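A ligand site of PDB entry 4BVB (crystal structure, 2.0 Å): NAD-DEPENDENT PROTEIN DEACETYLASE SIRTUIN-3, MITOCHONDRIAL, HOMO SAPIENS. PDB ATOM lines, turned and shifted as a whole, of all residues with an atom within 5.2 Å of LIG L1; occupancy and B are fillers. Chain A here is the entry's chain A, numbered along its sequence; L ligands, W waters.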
ATOM      1  N   GLY A  30     -12.729 -34.411  14.790  1.00  0.00           N
ATOM      2  CA  GLY A  30     -12.664 -33.465  15.906  1.00  0.00           C
ATOM      3  C   GLY A  30     -13.553 -32.238  15.592  1.00  0.00           C
ATOM      4  O   GLY A  30     -14.426 -32.274  14.683  1.00  0.00           O
ATOM      5  N   ALA A  31     -13.244 -31.119  16.252  1.00  0.00           N
ATOM      6  CA  ALA A  31     -14.145 -29.940  16.252  1.00  0.00           C
ATOM      7  C   ALA A  31     -14.286 -29.270  14.904  1.00  0.00           C
ATOM      8  O   ALA A  31     -15.325 -28.569  14.606  1.00  0.00           O
ATOM      9  CB  ALA A  31     -13.723 -28.931  17.317  1.00  0.00           C
ATOM     10  N   GLY A  32     -13.286 -29.516  14.051  1.00  0.00           N
ATOM     11  CA  GLY A  32     -13.332 -28.922  12.719  1.00  0.00           C
ATOM     12  C   GLY A  32     -14.481 -29.399  11.837  1.00  0.00           C
ATOM     13  O   GLY A  32     -14.832 -28.687  10.877  1.00  0.00           O
ATOM     14  N   THR A  35     -17.474 -26.867  12.845  1.00  0.00           N
ATOM     15  CA  THR A  35     -17.427 -25.464  12.478  1.00  0.00           C
ATOM     16  C   THR A  35     -18.397 -25.092  11.325  1.00  0.00           C
ATOM     17  O   THR A  35     -19.021 -24.031  11.378  1.00  0.00           O
ATOM     18  CB  THR A  35     -16.018 -24.956  12.219  1.00  0.00           C
ATOM     19  OG1 THR A  35     -15.451 -25.741  11.181  1.00  0.00           O
ATOM     20  CG2 THR A  35     -15.187 -25.122  13.452  1.00  0.00           C
ATOM     21  N   PRO A  36     -18.544 -25.954  10.294  1.00  0.00           N
ATOM     22  CA  PRO A  36     -19.630 -25.602   9.316  1.00  0.00           C
ATOM     23  C   PRO A  36     -21.067 -25.604   9.861  1.00  0.00           C
ATOM     24  O   PRO A  36     -21.910 -24.949   9.227  1.00  0.00           O
ATOM     25  CB  PRO A  36     -19.503 -26.691   8.243  1.00  0.00           C
ATOM     26  CG  PRO A  36     -18.058 -27.213   8.406  1.00  0.00           C
ATOM     27  CD  PRO A  36     -17.934 -27.258   9.935  1.00  0.00           C
ATOM     28  N   ASP A  41     -14.369 -24.393  16.887  1.00  0.00           N
ATOM     29  CA  ASP A  41     -13.347 -25.368  17.314  1.00  0.00           C
ATOM     30  C   ASP A  41     -12.561 -24.731  18.462  1.00  0.00           C
ATOM     31  O   ASP A  41     -12.986 -23.712  19.015  1.00  0.00           O
ATOM     32  CB  ASP A  41     -12.460 -25.763  16.107  1.00  0.00           C
ATOM     33  CG  ASP A  41     -11.582 -24.637  15.580  1.00  0.00           C
ATOM     34  OD1 ASP A  41     -11.476 -23.486  16.169  1.00  0.00           O
ATOM     35  OD2 ASP A  41     -11.024 -24.904  14.514  1.00  0.00           O
ATOM     36  N   PHE A  42     -11.413 -25.275  18.798  1.00  0.00           N
ATOM     37  CA  PHE A  42     -10.695 -24.715  19.901  1.00  0.00           C
ATOM     38  C   PHE A  42      -9.608 -23.770  19.508  1.00  0.00           C
ATOM     39  O   PHE A  42      -9.434 -22.704  20.171  1.00  0.00           O
ATOM     40  CB  PHE A  42     -10.112 -25.836  20.780  1.00  0.00           C
ATOM     41  CG  PHE A  42     -11.136 -26.585  21.544  1.00  0.00           C
ATOM     42  CD1 PHE A  42     -11.716 -27.718  21.000  1.00  0.00           C
ATOM     43  CD2 PHE A  42     -11.420 -26.237  22.861  1.00  0.00           C
ATOM     44  CE1 PHE A  42     -12.684 -28.448  21.756  1.00  0.00           C
ATOM     45  CE2 PHE A  42     -12.340 -26.958  23.621  1.00  0.00           C
ATOM     46  CZ  PHE A  42     -12.989 -28.061  23.028  1.00  0.00           C
ATOM     47  N   ARG A  43      -8.902 -24.097  18.427  1.00  0.00           N
ATOM     48  CA  ARG A  43      -7.577 -23.597  18.181  1.00  0.00           C
ATOM     49  C   ARG A  43      -7.494 -22.690  16.932  1.00  0.00           C
ATOM     50  O   ARG A  43      -6.447 -22.121  16.727  1.00  0.00           O
ATOM     51  CB  ARG A  43      -6.559 -24.786  18.085  1.00  0.00           C
ATOM     52  CG  ARG A  43      -6.376 -25.553  19.411  1.00  0.00           C
ATOM     53  CD  ARG A  43      -5.431 -26.794  19.417  1.00  0.00           C
ATOM     54  NE  ARG A  43      -5.339 -27.278  20.845  1.00  0.00           N
ATOM     55  CZ  ARG A  43      -6.215 -28.085  21.473  1.00  0.00           C
ATOM     56  NH1 ARG A  43      -7.283 -28.631  20.860  1.00  0.00           N
ATOM     57  NH2 ARG A  43      -6.020 -28.411  22.757  1.00  0.00           N
ATOM     58  N   SER A  44      -8.556 -22.552  16.128  1.00  0.00           N
ATOM     59  CA  SER A  44      -8.477 -21.708  14.976  1.00  0.00           C
ATOM     60  C   SER A  44      -8.219 -20.280  15.445  1.00  0.00           C
ATOM     61  O   SER A  44      -8.888 -19.825  16.409  1.00  0.00           O
ATOM     62  CB  SER A  44      -9.730 -21.773  14.132  1.00  0.00           C
ATOM     63  OG  SER A  44      -9.797 -23.063  13.482  1.00  0.00           O
ATOM     64  N   TYR A  50     -10.539 -20.878  22.286  1.00  0.00           N
ATOM     65  CA  TYR A  50      -9.470 -20.390  23.164  1.00  0.00           C
ATOM     66  C   TYR A  50      -9.260 -18.923  23.117  1.00  0.00           C
ATOM     67  O   TYR A  50      -8.765 -18.345  24.046  1.00  0.00           O
ATOM     68  CB  TYR A  50      -8.152 -21.053  22.833  1.00  0.00           C
ATOM     69  CG  TYR A  50      -8.151 -22.435  23.367  1.00  0.00           C
ATOM     70  CD1 TYR A  50      -9.011 -22.786  24.369  1.00  0.00           C
ATOM     71  CD2 TYR A  50      -7.327 -23.410  22.816  1.00  0.00           C
ATOM     72  CE1 TYR A  50      -9.067 -24.054  24.841  1.00  0.00           C
ATOM     73  CE2 TYR A  50      -7.367 -24.700  23.304  1.00  0.00           C
ATOM     74  CZ  TYR A  50      -8.224 -25.003  24.331  1.00  0.00           C
ATOM     75  OH  TYR A  50      -8.287 -26.294  24.840  1.00  0.00           O
ATOM     76  N   GLN A 113     -13.994 -36.877  18.984  1.00  0.00           N
ATOM     77  CA  GLN A 113     -13.698 -36.034  20.121  1.00  0.00           C
ATOM     78  C   GLN A 113     -14.760 -35.028  20.426  1.00  0.00           C
ATOM     79  O   GLN A 113     -14.578 -34.274  21.362  1.00  0.00           O
ATOM     80  CB  GLN A 113     -12.397 -35.297  19.838  1.00  0.00           C
ATOM     81  CG  GLN A 113     -11.275 -36.311  19.666  1.00  0.00           C
ATOM     82  CD  GLN A 113     -10.066 -35.673  18.957  1.00  0.00           C
ATOM     83  OE1 GLN A 113      -9.065 -35.343  19.608  1.00  0.00           O
ATOM     84  NE2 GLN A 113     -10.192 -35.450  17.633  1.00  0.00           N
ATOM     85  N   ASN A 114     -15.841 -34.975  19.621  1.00  0.00           N
ATOM     86  CA  ASN A 114     -16.857 -33.935  19.825  1.00  0.00           C
ATOM     87  C   ASN A 114     -17.920 -34.338  20.814  1.00  0.00           C
ATOM     88  O   ASN A 114     -18.237 -35.534  20.920  1.00  0.00           O
ATOM     89  CB  ASN A 114     -17.544 -33.514  18.509  1.00  0.00           C
ATOM     90  CG  ASN A 114     -16.568 -32.906  17.501  1.00  0.00           C
ATOM     91  OD1 ASN A 114     -15.424 -32.570  17.866  1.00  0.00           O
ATOM     92  ND2 ASN A 114     -16.994 -32.854  16.195  1.00  0.00           N
ATOM     93  N   HIS A 133     -14.889 -38.269  23.980  1.00  0.00           N
ATOM     94  CA  HIS A 133     -14.946 -37.209  25.019  1.00  0.00           C
ATOM     95  C   HIS A 133     -16.290 -37.089  25.732  1.00  0.00           C
ATOM     96  O   HIS A 133     -16.579 -36.048  26.362  1.00  0.00           O
ATOM     97  CB  HIS A 133     -14.447 -35.842  24.478  1.00  0.00           C
ATOM     98  CG  HIS A 133     -12.986 -35.845  24.152  1.00  0.00           C
ATOM     99  ND1 HIS A 133     -12.379 -34.854  23.435  1.00  0.00           N
ATOM    100  CD2 HIS A 133     -12.029 -36.759  24.405  1.00  0.00           C
ATOM    101  CE1 HIS A 133     -11.098 -35.137  23.273  1.00  0.00           C
ATOM    102  NE2 HIS A 133     -10.860 -36.292  23.858  1.00  0.00           N
ATOM    103  N   VAL A 177     -15.971 -35.400  29.023  1.00  0.00           N
ATOM    104  CA  VAL A 177     -14.646 -35.664  29.550  1.00  0.00           C
ATOM    105  C   VAL A 177     -13.869 -34.361  29.622  1.00  0.00           C
ATOM    106  O   VAL A 177     -13.393 -33.831  28.583  1.00  0.00           O
ATOM    107  CB  VAL A 177     -13.892 -36.656  28.651  1.00  0.00           C
ATOM    108  CG1 VAL A 177     -12.451 -36.840  29.157  1.00  0.00           C
ATOM    109  CG2 VAL A 177     -14.670 -38.014  28.604  1.00  0.00           C
ATOM    110  N   PHE A 179     -10.783 -31.836  30.347  1.00  0.00           N
ATOM    111  CA  PHE A 179      -9.403 -31.962  29.859  1.00  0.00           C
ATOM    112  C   PHE A 179      -8.565 -32.728  30.875  1.00  0.00           C
ATOM    113  O   PHE A 179      -8.552 -32.366  32.046  1.00  0.00           O
ATOM    114  CB  PHE A 179      -8.786 -30.592  29.615  1.00  0.00           C
ATOM    115  CG  PHE A 179      -9.319 -29.864  28.411  1.00  0.00           C
ATOM    116  CD1 PHE A 179     -10.489 -30.316  27.713  1.00  0.00           C
ATOM    117  CD2 PHE A 179      -8.684 -28.681  27.974  1.00  0.00           C
ATOM    118  CE1 PHE A 179     -10.953 -29.634  26.597  1.00  0.00           C
ATOM    119  CE2 PHE A 179      -9.159 -27.990  26.861  1.00  0.00           C
ATOM    120  CZ  PHE A 179     -10.283 -28.491  26.167  1.00  0.00           C
ATOM    121  N   GLY A 204     -10.983 -32.846  10.369  1.00  0.00           N
ATOM    122  CA  GLY A 204     -11.304 -31.693  11.262  1.00  0.00           C
ATOM    123  C   GLY A 204     -10.770 -31.887  12.680  1.00  0.00           C
ATOM    124  O   GLY A 204     -11.494 -31.666  13.622  1.00  0.00           O
ATOM    125  N   THR A 205      -9.525 -32.295  12.826  1.00  0.00           N
ATOM    126  CA  THR A 205      -8.899 -32.377  14.129  1.00  0.00           C
ATOM    127  C   THR A 205      -7.432 -31.905  13.962  1.00  0.00           C
ATOM    128  O   THR A 205      -6.804 -32.141  12.931  1.00  0.00           O
ATOM    129  CB  THR A 205      -9.014 -33.739  14.815  1.00  0.00           C
ATOM    130  OG1 THR A 205      -8.212 -33.745  16.026  1.00  0.00           O
ATOM    131  CG2 THR A 205      -8.511 -34.909  13.893  1.00  0.00           C
ATOM    132  N   SER A 206      -6.937 -31.157  14.956  1.00  0.00           N
ATOM    133  CA  SER A 206      -5.526 -30.757  15.013  1.00  0.00           C
ATOM    134  C   SER A 206      -4.604 -31.938  15.466  1.00  0.00           C
ATOM    135  O   SER A 206      -3.339 -31.848  15.357  1.00  0.00           O
ATOM    136  CB  SER A 206      -5.399 -29.628  16.025  1.00  0.00           C
ATOM    137  OG  SER A 206      -5.642 -30.134  17.376  1.00  0.00           O
ATOM    138  N   LEU A 207      -5.179 -33.003  16.017  1.00  0.00           N
ATOM    139  CA  LEU A 207      -4.337 -34.168  16.454  1.00  0.00           C
ATOM    140  C   LEU A 207      -3.229 -33.738  17.454  1.00  0.00           C
ATOM    141  O   LEU A 207      -2.103 -34.223  17.381  1.00  0.00           O
ATOM    142  CB  LEU A 207      -3.722 -34.884  15.261  1.00  0.00           C
ATOM    143  CG  LEU A 207      -4.652 -35.606  14.261  1.00  0.00           C
ATOM    144  CD1 LEU A 207      -3.899 -36.330  13.140  1.00  0.00           C
ATOM    145  CD2 LEU A 207      -5.597 -36.585  14.974  1.00  0.00           C
ATOM    146  N   GLU A 208      -3.558 -32.782  18.332  1.00  0.00           N
ATOM    147  CA  GLU A 208      -2.685 -32.333  19.460  1.00  0.00           C
ATOM    148  C   GLU A 208      -2.899 -33.178  20.711  1.00  0.00           C
ATOM    149  O   GLU A 208      -1.979 -33.400  21.497  1.00  0.00           O
ATOM    150  CB  GLU A 208      -3.069 -30.920  19.892  1.00  0.00           C
ATOM    151  CG  GLU A 208      -3.047 -29.867  18.821  1.00  0.00           C
ATOM    152  CD  GLU A 208      -1.720 -29.197  18.641  1.00  0.00           C
ATOM    153  OE1 GLU A 208      -0.773 -29.461  19.418  1.00  0.00           O
ATOM    154  OE2 GLU A 208      -1.625 -28.408  17.702  1.00  0.00           O
ATOM    155  N   VAL A 209      -4.121 -33.635  20.913  1.00  0.00           N
ATOM    156  CA  VAL A 209      -4.499 -34.154  22.198  1.00  0.00           C
ATOM    157  C   VAL A 209      -4.388 -35.687  22.121  1.00  0.00           C
ATOM    158  O   VAL A 209      -4.952 -36.299  21.195  1.00  0.00           O
ATOM    159  CB  VAL A 209      -5.906 -33.584  22.547  1.00  0.00           C
ATOM    160  CG1 VAL A 209      -6.421 -34.092  23.867  1.00  0.00           C
ATOM    161  CG2 VAL A 209      -5.836 -32.038  22.599  1.00  0.00           C
ATOM    162  N   ASN A 229      -8.688 -31.814   6.136  1.00  0.00           N
ATOM    163  CA  ASN A 229      -8.522 -30.839   7.211  1.00  0.00           C
ATOM    164  C   ASN A 229      -7.936 -29.567   6.603  1.00  0.00           C
ATOM    165  O   ASN A 229      -7.356 -29.639   5.514  1.00  0.00           O
ATOM    166  CB  ASN A 229      -7.547 -31.378   8.276  1.00  0.00           C
ATOM    167  CG  ASN A 229      -7.674 -30.664   9.621  1.00  0.00           C
ATOM    168  OD1 ASN A 229      -8.809 -30.525  10.144  1.00  0.00           O
ATOM    169  ND2 ASN A 229      -6.545 -30.203  10.208  1.00  0.00           N
ATOM    170  N   ARG A 230      -8.088 -28.422   7.288  1.00  0.00           N
ATOM    171  CA  ARG A 230      -7.370 -27.187   6.924  1.00  0.00           C
ATOM    172  C   ARG A 230      -5.863 -27.398   6.736  1.00  0.00           C
ATOM    173  O   ARG A 230      -5.272 -26.915   5.778  1.00  0.00           O
ATOM    174  CB  ARG A 230      -7.591 -26.106   8.001  1.00  0.00           C
ATOM    175  CG  ARG A 230      -6.783 -24.821   7.762  1.00  0.00           C
ATOM    176  CD  ARG A 230      -7.176 -24.230   6.414  1.00  0.00           C
ATOM    177  NE  ARG A 230      -8.635 -24.110   6.354  1.00  0.00           N
ATOM    178  CZ  ARG A 230      -9.334 -23.824   5.267  1.00  0.00           C
ATOM    179  NH1 ARG A 230      -8.723 -23.586   4.108  1.00  0.00           N
ATOM    180  NH2 ARG A 230     -10.650 -23.711   5.378  1.00  0.00           N
ATOM    181  N   ASP A 231      -5.227 -28.075   7.680  1.00  0.00           N
ATOM    182  CA  ASP A 231      -3.753 -28.225   7.660  1.00  0.00           C
ATOM    183  C   ASP A 231      -3.301 -29.663   7.848  1.00  0.00           C
ATOM    184  O   ASP A 231      -4.008 -30.451   8.430  1.00  0.00           O
ATOM    185  CB  ASP A 231      -3.055 -27.509   8.809  1.00  0.00           C
ATOM    186  CG  ASP A 231      -3.651 -26.226   9.145  1.00  0.00           C
ATOM    187  OD1 ASP A 231      -3.553 -25.293   8.293  1.00  0.00           O
ATOM    188  OD2 ASP A 231      -4.205 -26.152  10.273  1.00  0.00           O
ATOM    189  N   VAL A 233      -1.363 -32.240   9.915  1.00  0.00           N
ATOM    190  CA  VAL A 233      -1.211 -32.188  11.352  1.00  0.00           C
ATOM    191  C   VAL A 233      -0.819 -33.486  12.041  1.00  0.00           C
ATOM    192  O   VAL A 233      -1.057 -34.565  11.510  1.00  0.00           O
ATOM    193  CB  VAL A 233      -2.530 -31.716  12.065  1.00  0.00           C
ATOM    194  CG1 VAL A 233      -2.857 -30.237  11.704  1.00  0.00           C
ATOM    195  CG2 VAL A 233      -3.732 -32.628  11.713  1.00  0.00           C
ATOM    196  N   GLY A 249      -7.687 -27.983   3.031  1.00  0.00           N
ATOM    197  CA  GLY A 249      -8.688 -26.965   2.666  1.00  0.00           C
ATOM    198  C   GLY A 249      -9.948 -27.152   3.518  1.00  0.00           C
ATOM    199  O   GLY A 249      -9.944 -27.927   4.500  1.00  0.00           O
ATOM    200  N   ASP A 250     -10.996 -26.392   3.213  1.00  0.00           N
ATOM    201  CA  ASP A 250     -12.241 -26.472   3.940  1.00  0.00           C
ATOM    202  C   ASP A 250     -12.705 -27.944   3.955  1.00  0.00           C
ATOM    203  O   ASP A 250     -12.638 -28.660   2.897  1.00  0.00           O
ATOM    204  CB  ASP A 250     -13.303 -25.583   3.260  1.00  0.00           C
ATOM    205  CG  ASP A 250     -14.651 -25.733   3.907  1.00  0.00           C
ATOM    206  OD1 ASP A 250     -14.924 -25.185   4.990  1.00  0.00           O
ATOM    207  OD2 ASP A 250     -15.453 -26.485   3.373  1.00  0.00           O
ATOM    208  N   VAL A 251     -13.215 -28.387   5.095  1.00  0.00           N
ATOM    209  CA  VAL A 251     -13.611 -29.804   5.245  1.00  0.00           C
ATOM    210  C   VAL A 251     -14.843 -30.196   4.411  1.00  0.00           C
ATOM    211  O   VAL A 251     -14.914 -31.334   3.888  1.00  0.00           O
ATOM    212  CB  VAL A 251     -13.800 -30.233   6.716  1.00  0.00           C
ATOM    213  CG1 VAL A 251     -15.045 -29.553   7.350  1.00  0.00           C
ATOM    214  CG2 VAL A 251     -13.859 -31.763   6.823  1.00  0.00           C
ATOM    215  N   VAL A 252     -15.767 -29.250   4.253  1.00  0.00           N
ATOM    216  CA  VAL A 252     -16.945 -29.514   3.408  1.00  0.00           C
ATOM    217  C   VAL A 252     -16.551 -29.625   1.955  1.00  0.00           C
ATOM    218  O   VAL A 252     -17.007 -30.508   1.281  1.00  0.00           O
ATOM    219  CB  VAL A 252     -18.095 -28.469   3.615  1.00  0.00           C
ATOM    220  CG1 VAL A 252     -19.172 -28.627   2.530  1.00  0.00           C
ATOM    221  CG2 VAL A 252     -18.739 -28.633   5.022  1.00  0.00           C
HETATM  222  N1  LIG L   1     -12.341 -26.995   7.361  1.00  0.00           N
HETATM  223  C1  LIG L   1     -11.160 -27.664   7.497  1.00  0.00           C
HETATM  224  N2  LIG L   1     -10.542 -27.750   8.677  1.00  0.00           N
HETATM  225  C2  LIG L   1     -11.055 -27.131   9.765  1.00  0.00           C
HETATM  226  C3  LIG L   1     -12.277 -26.352   9.649  1.00  0.00           C
HETATM  227  C4  LIG L   1     -12.916 -26.323   8.363  1.00  0.00           C
HETATM  228  N3  LIG L   1     -14.077 -25.658   8.181  1.00  0.00           N
HETATM  229  N4  LIG L   1     -12.540 -25.796  10.879  1.00  0.00           N
HETATM  230  C5  LIG L   1     -11.532 -26.214  11.696  1.00  0.00           C
HETATM  231  N5  LIG L   1     -10.644 -26.956  11.030  1.00  0.00           N
HETATM  232  P1  LIG L   1      -8.926 -28.283  17.401  1.00  0.00           P
HETATM  233  P2  LIG L   1      -9.904 -30.933  18.128  1.00  0.00           P
HETATM  234  C6  LIG L   1      -9.481 -27.604  11.591  1.00  0.00           C
HETATM  235  O1  LIG L   1      -9.589 -26.936  17.444  1.00  0.00           O
HETATM  236  O2  LIG L   1     -11.297 -31.502  18.112  1.00  0.00           O
HETATM  237  C7  LIG L   1      -9.767 -30.308  23.577  1.00  0.00           C
HETATM  238  O3  LIG L   1      -9.114 -30.893  24.746  1.00  0.00           O
HETATM  239  C8  LIG L   1      -8.592 -26.639  12.351  1.00  0.00           C
HETATM  240  O4  LIG L   1      -7.705 -26.138  11.316  1.00  0.00           O
HETATM  241  O5  LIG L   1      -7.690 -28.625  18.216  1.00  0.00           O
HETATM  242  O6  LIG L   1      -8.807 -31.510  17.284  1.00  0.00           O
HETATM  243  C9  LIG L   1     -11.079 -31.025  23.527  1.00  0.00           C
HETATM  244  O7  LIG L   1     -10.909 -32.218  24.355  1.00  0.00           O
HETATM  245  C10 LIG L   1      -7.922 -27.599  13.314  1.00  0.00           C
HETATM  246  O8  LIG L   1      -6.882 -28.285  12.594  1.00  0.00           O
HETATM  247  O9  LIG L   1     -10.059 -29.331  17.875  1.00  0.00           O
HETATM  248  C11 LIG L   1     -11.173 -31.464  22.077  1.00  0.00           C
HETATM  249  O10 LIG L   1     -11.945 -32.664  21.840  1.00  0.00           O
HETATM  250  C12 LIG L   1      -9.006 -28.661  13.571  1.00  0.00           C
HETATM  251  O11 LIG L   1     -10.014 -28.513  12.559  1.00  0.00           O
HETATM  252  C13 LIG L   1      -9.740 -31.638  21.646  1.00  0.00           C
HETATM  253  O12 LIG L   1      -8.991 -30.779  22.478  1.00  0.00           O
HETATM  254  C14 LIG L   1      -9.698 -28.392  14.925  1.00  0.00           C
HETATM  255  O13 LIG L   1      -8.643 -28.520  15.877  1.00  0.00           O
HETATM  256  C15 LIG L   1      -9.871 -30.672  20.480  1.00  0.00           C
HETATM  257  O14 LIG L   1      -9.255 -31.353  19.505  1.00  0.00           O
HETATM  258  N1  LG2 L   2     -17.840 -29.660  18.543  1.00  0.00           N
HETATM  259  O1  LG2 L   2     -18.158 -30.942  20.352  1.00  0.00           O
HETATM  260  C1  LG2 L   2     -17.505 -30.076  19.754  1.00  0.00           C
HETATM  261  N2  LG2 L   2     -15.359 -31.126  22.055  1.00  0.00           N
HETATM  262  C2  LG2 L   2     -16.811 -27.861  22.877  1.00  0.00           C
HETATM  263  C3  LG2 L   2     -14.735 -32.056  24.235  1.00  0.00           C
HETATM  264  C4  LG2 L   2     -14.634 -31.844  25.591  1.00  0.00           C
HETATM  265  C5  LG2 L   2     -15.205 -31.103  23.406  1.00  0.00           C
HETATM  266 CL1  LG2 L   2     -14.998 -30.387  27.920  1.00  0.00          CL
HETATM  267  C6  LG2 L   2     -15.732 -29.956  23.902  1.00  0.00           C
HETATM  268  C7  LG2 L   2     -15.671 -29.691  25.233  1.00  0.00           C
HETATM  269  C8  LG2 L   2     -16.231 -29.226  22.873  1.00  0.00           C
HETATM  270  C9  LG2 L   2     -15.984 -29.956  21.711  1.00  0.00           C
HETATM  271  C10 LG2 L   2     -15.121 -30.646  26.122  1.00  0.00           C
HETATM  272  C11 LG2 L   2     -17.325 -27.435  21.389  1.00  0.00           C
HETATM  273  C12 LG2 L   2     -16.300 -29.478  20.365  1.00  0.00           C
HETATM  274  C13 LG2 L   2     -16.294 -27.873  20.363  1.00  0.00           C
HETATM  275  O   HOH W   1      -4.418 -26.988  13.096  1.00  0.00           O
HETATM  276  O   HOH W   2     -11.054 -34.458  27.007  1.00  0.00           O
HETATM  277  O   HOH W   3     -13.369 -31.743  19.611  1.00  0.00           O
HETATM  278  O   HOH W   4      -9.275 -32.899  26.245  1.00  0.00           O
HETATM  279  O   HOH W   5      -6.162 -32.310  18.976  1.00  0.00           O
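Merely in contact with LIG L1: Gly 30, Gly 32, Asp 41, Ser 44, Phe 179, Gly 204, Val 209, Asp 231 and Gly 249. Hydrophobic or aromatic side chains that line LIG L1: Ala 31, Phe 42, His 133, Phe 179, Val 209 and Val 251. 21 residues have an atom within 4 Å of LIG L1: Gly 30, Ala 31, Gly 32, Thr 35, Asp 41, Phe 42, Arg 43, Ser 44, Gln 113, His 133, Phe 179, Gly 204, Thr 205, Ser 206, Val 209, Asn 229, Arg 230, Asp 231, Gly 249, Asp 250 and Val 251. The nearest printed residue that does not touch LIG L1 is Leu 207 (4.1 Å).
The side-chain hydroxyl (OG1) of Thr 205 is in hydrogen-bond range of an oxygen (O6) of LIG L1, 2.6 Å away. An oxygen (O1) of LIG L1 is in hydrogen-bond range of the backbone NH (N) of Arg 43, at 3.1 Å. An oxygen (O5) of LIG L1 lies within salt-bridge range of the guanidinium group (NH1) of Arg 43, 2.7 Å away. O6 of LIG L1 lies within hydrogen-bond range of N of Ser 206 (3.0 Å). OG of Ser 206 lies within hydrogen-bond range of O5 of LIG L1. N of Ala 31 is in hydrogen-bond range of O2 of LIG L1 (2.7 Å). An oxygen (O10) of LIG L1 is in hydrogen-bond range of a ring nitrogen (ND1) of His 133 (2.7 Å). The backbone NH (N) of Val 251 is in hydrogen-bond range of a nitrogen (N1) of LIG L1 (2.8 Å). The backbone NH (N) of Phe 42 is in hydrogen-bond range of an oxygen (O1) of LIG L1, at 2.8 Å. The backbone NH of Arg 230 is in hydrogen-bond range of a nitrogen (N2) of LIG L1. The side-chain hydroxyl (OG1) of Thr 35 lies within hydrogen-bond range of a nitrogen (N4) of LIG L1 (2.9 Å). ND2 of Asn 229 sits at hydrogen-bond distance from O8 of LIG L1 (3.1 Å). O10 of LIG L1 lies within hydrogen-bond range of O of Gln 113, at 3.1 Å. The side-chain carboxylate (OD1) of Asp 250 sits at hydrogen-bond distance from a nitrogen (N3) of LIG L1 (3.3 Å). The backbone carbonyl oxygen (O) of Gln 113 is in hydrogen-bond range of a nitrogen (N2) of LG2 L2.
N of Thr 205 sits at hydrogen-bond distance from OD1 of Asn 229 (3.3 Å). N of Arg 43 sits at hydrogen-bond distance from OD1 of Asp 41 (3.5 Å). The backbone NH (N) of Ala 31 is in hydrogen-bond range of the side-chain amide oxygen (OD1) of Asn 114. N of Gly 204 sits close to OD1 of Asn 229, at 3.2 Å. The side-chain carboxylate of Asp 41 sits at hydrogen-bond distance from the side-chain hydroxyl of Ser 44. The backbone NH of Gly 30 lies close to the backbone carbonyl oxygen of Gly 204 (3.2 Å). The backbone carbonyl oxygen of Gly 30 sits at hydrogen-bond distance from the side-chain amide nitrogen of Asn 114 (3.0 Å). The backbone NH (N) of Gly 32 lies within hydrogen-bond range of the backbone carbonyl oxygen (O) of Gly 204.
Water W3 lies within hydrogen-bond range of an oxygen (O2) of LIG L1 (2.6 Å), the side-chain amide oxygen (OD1) of Asn 114 (2.8 Å), a nitrogen (N2) of LG2 L2 (3.2 Å), the backbone carbonyl oxygen (O) of Gln 113 (3.3 Å) and the backbone NH (N) of Ala 31 (3.4 Å). Water W1 bridges O8 of LIG L1 (2.8 Å) and OD2 of Asp 231 (3.0 Å). Water W2 lies within hydrogen-bond range of the backbone carbonyl oxygen of Val 177 and an oxygen (O7) of LIG L1.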
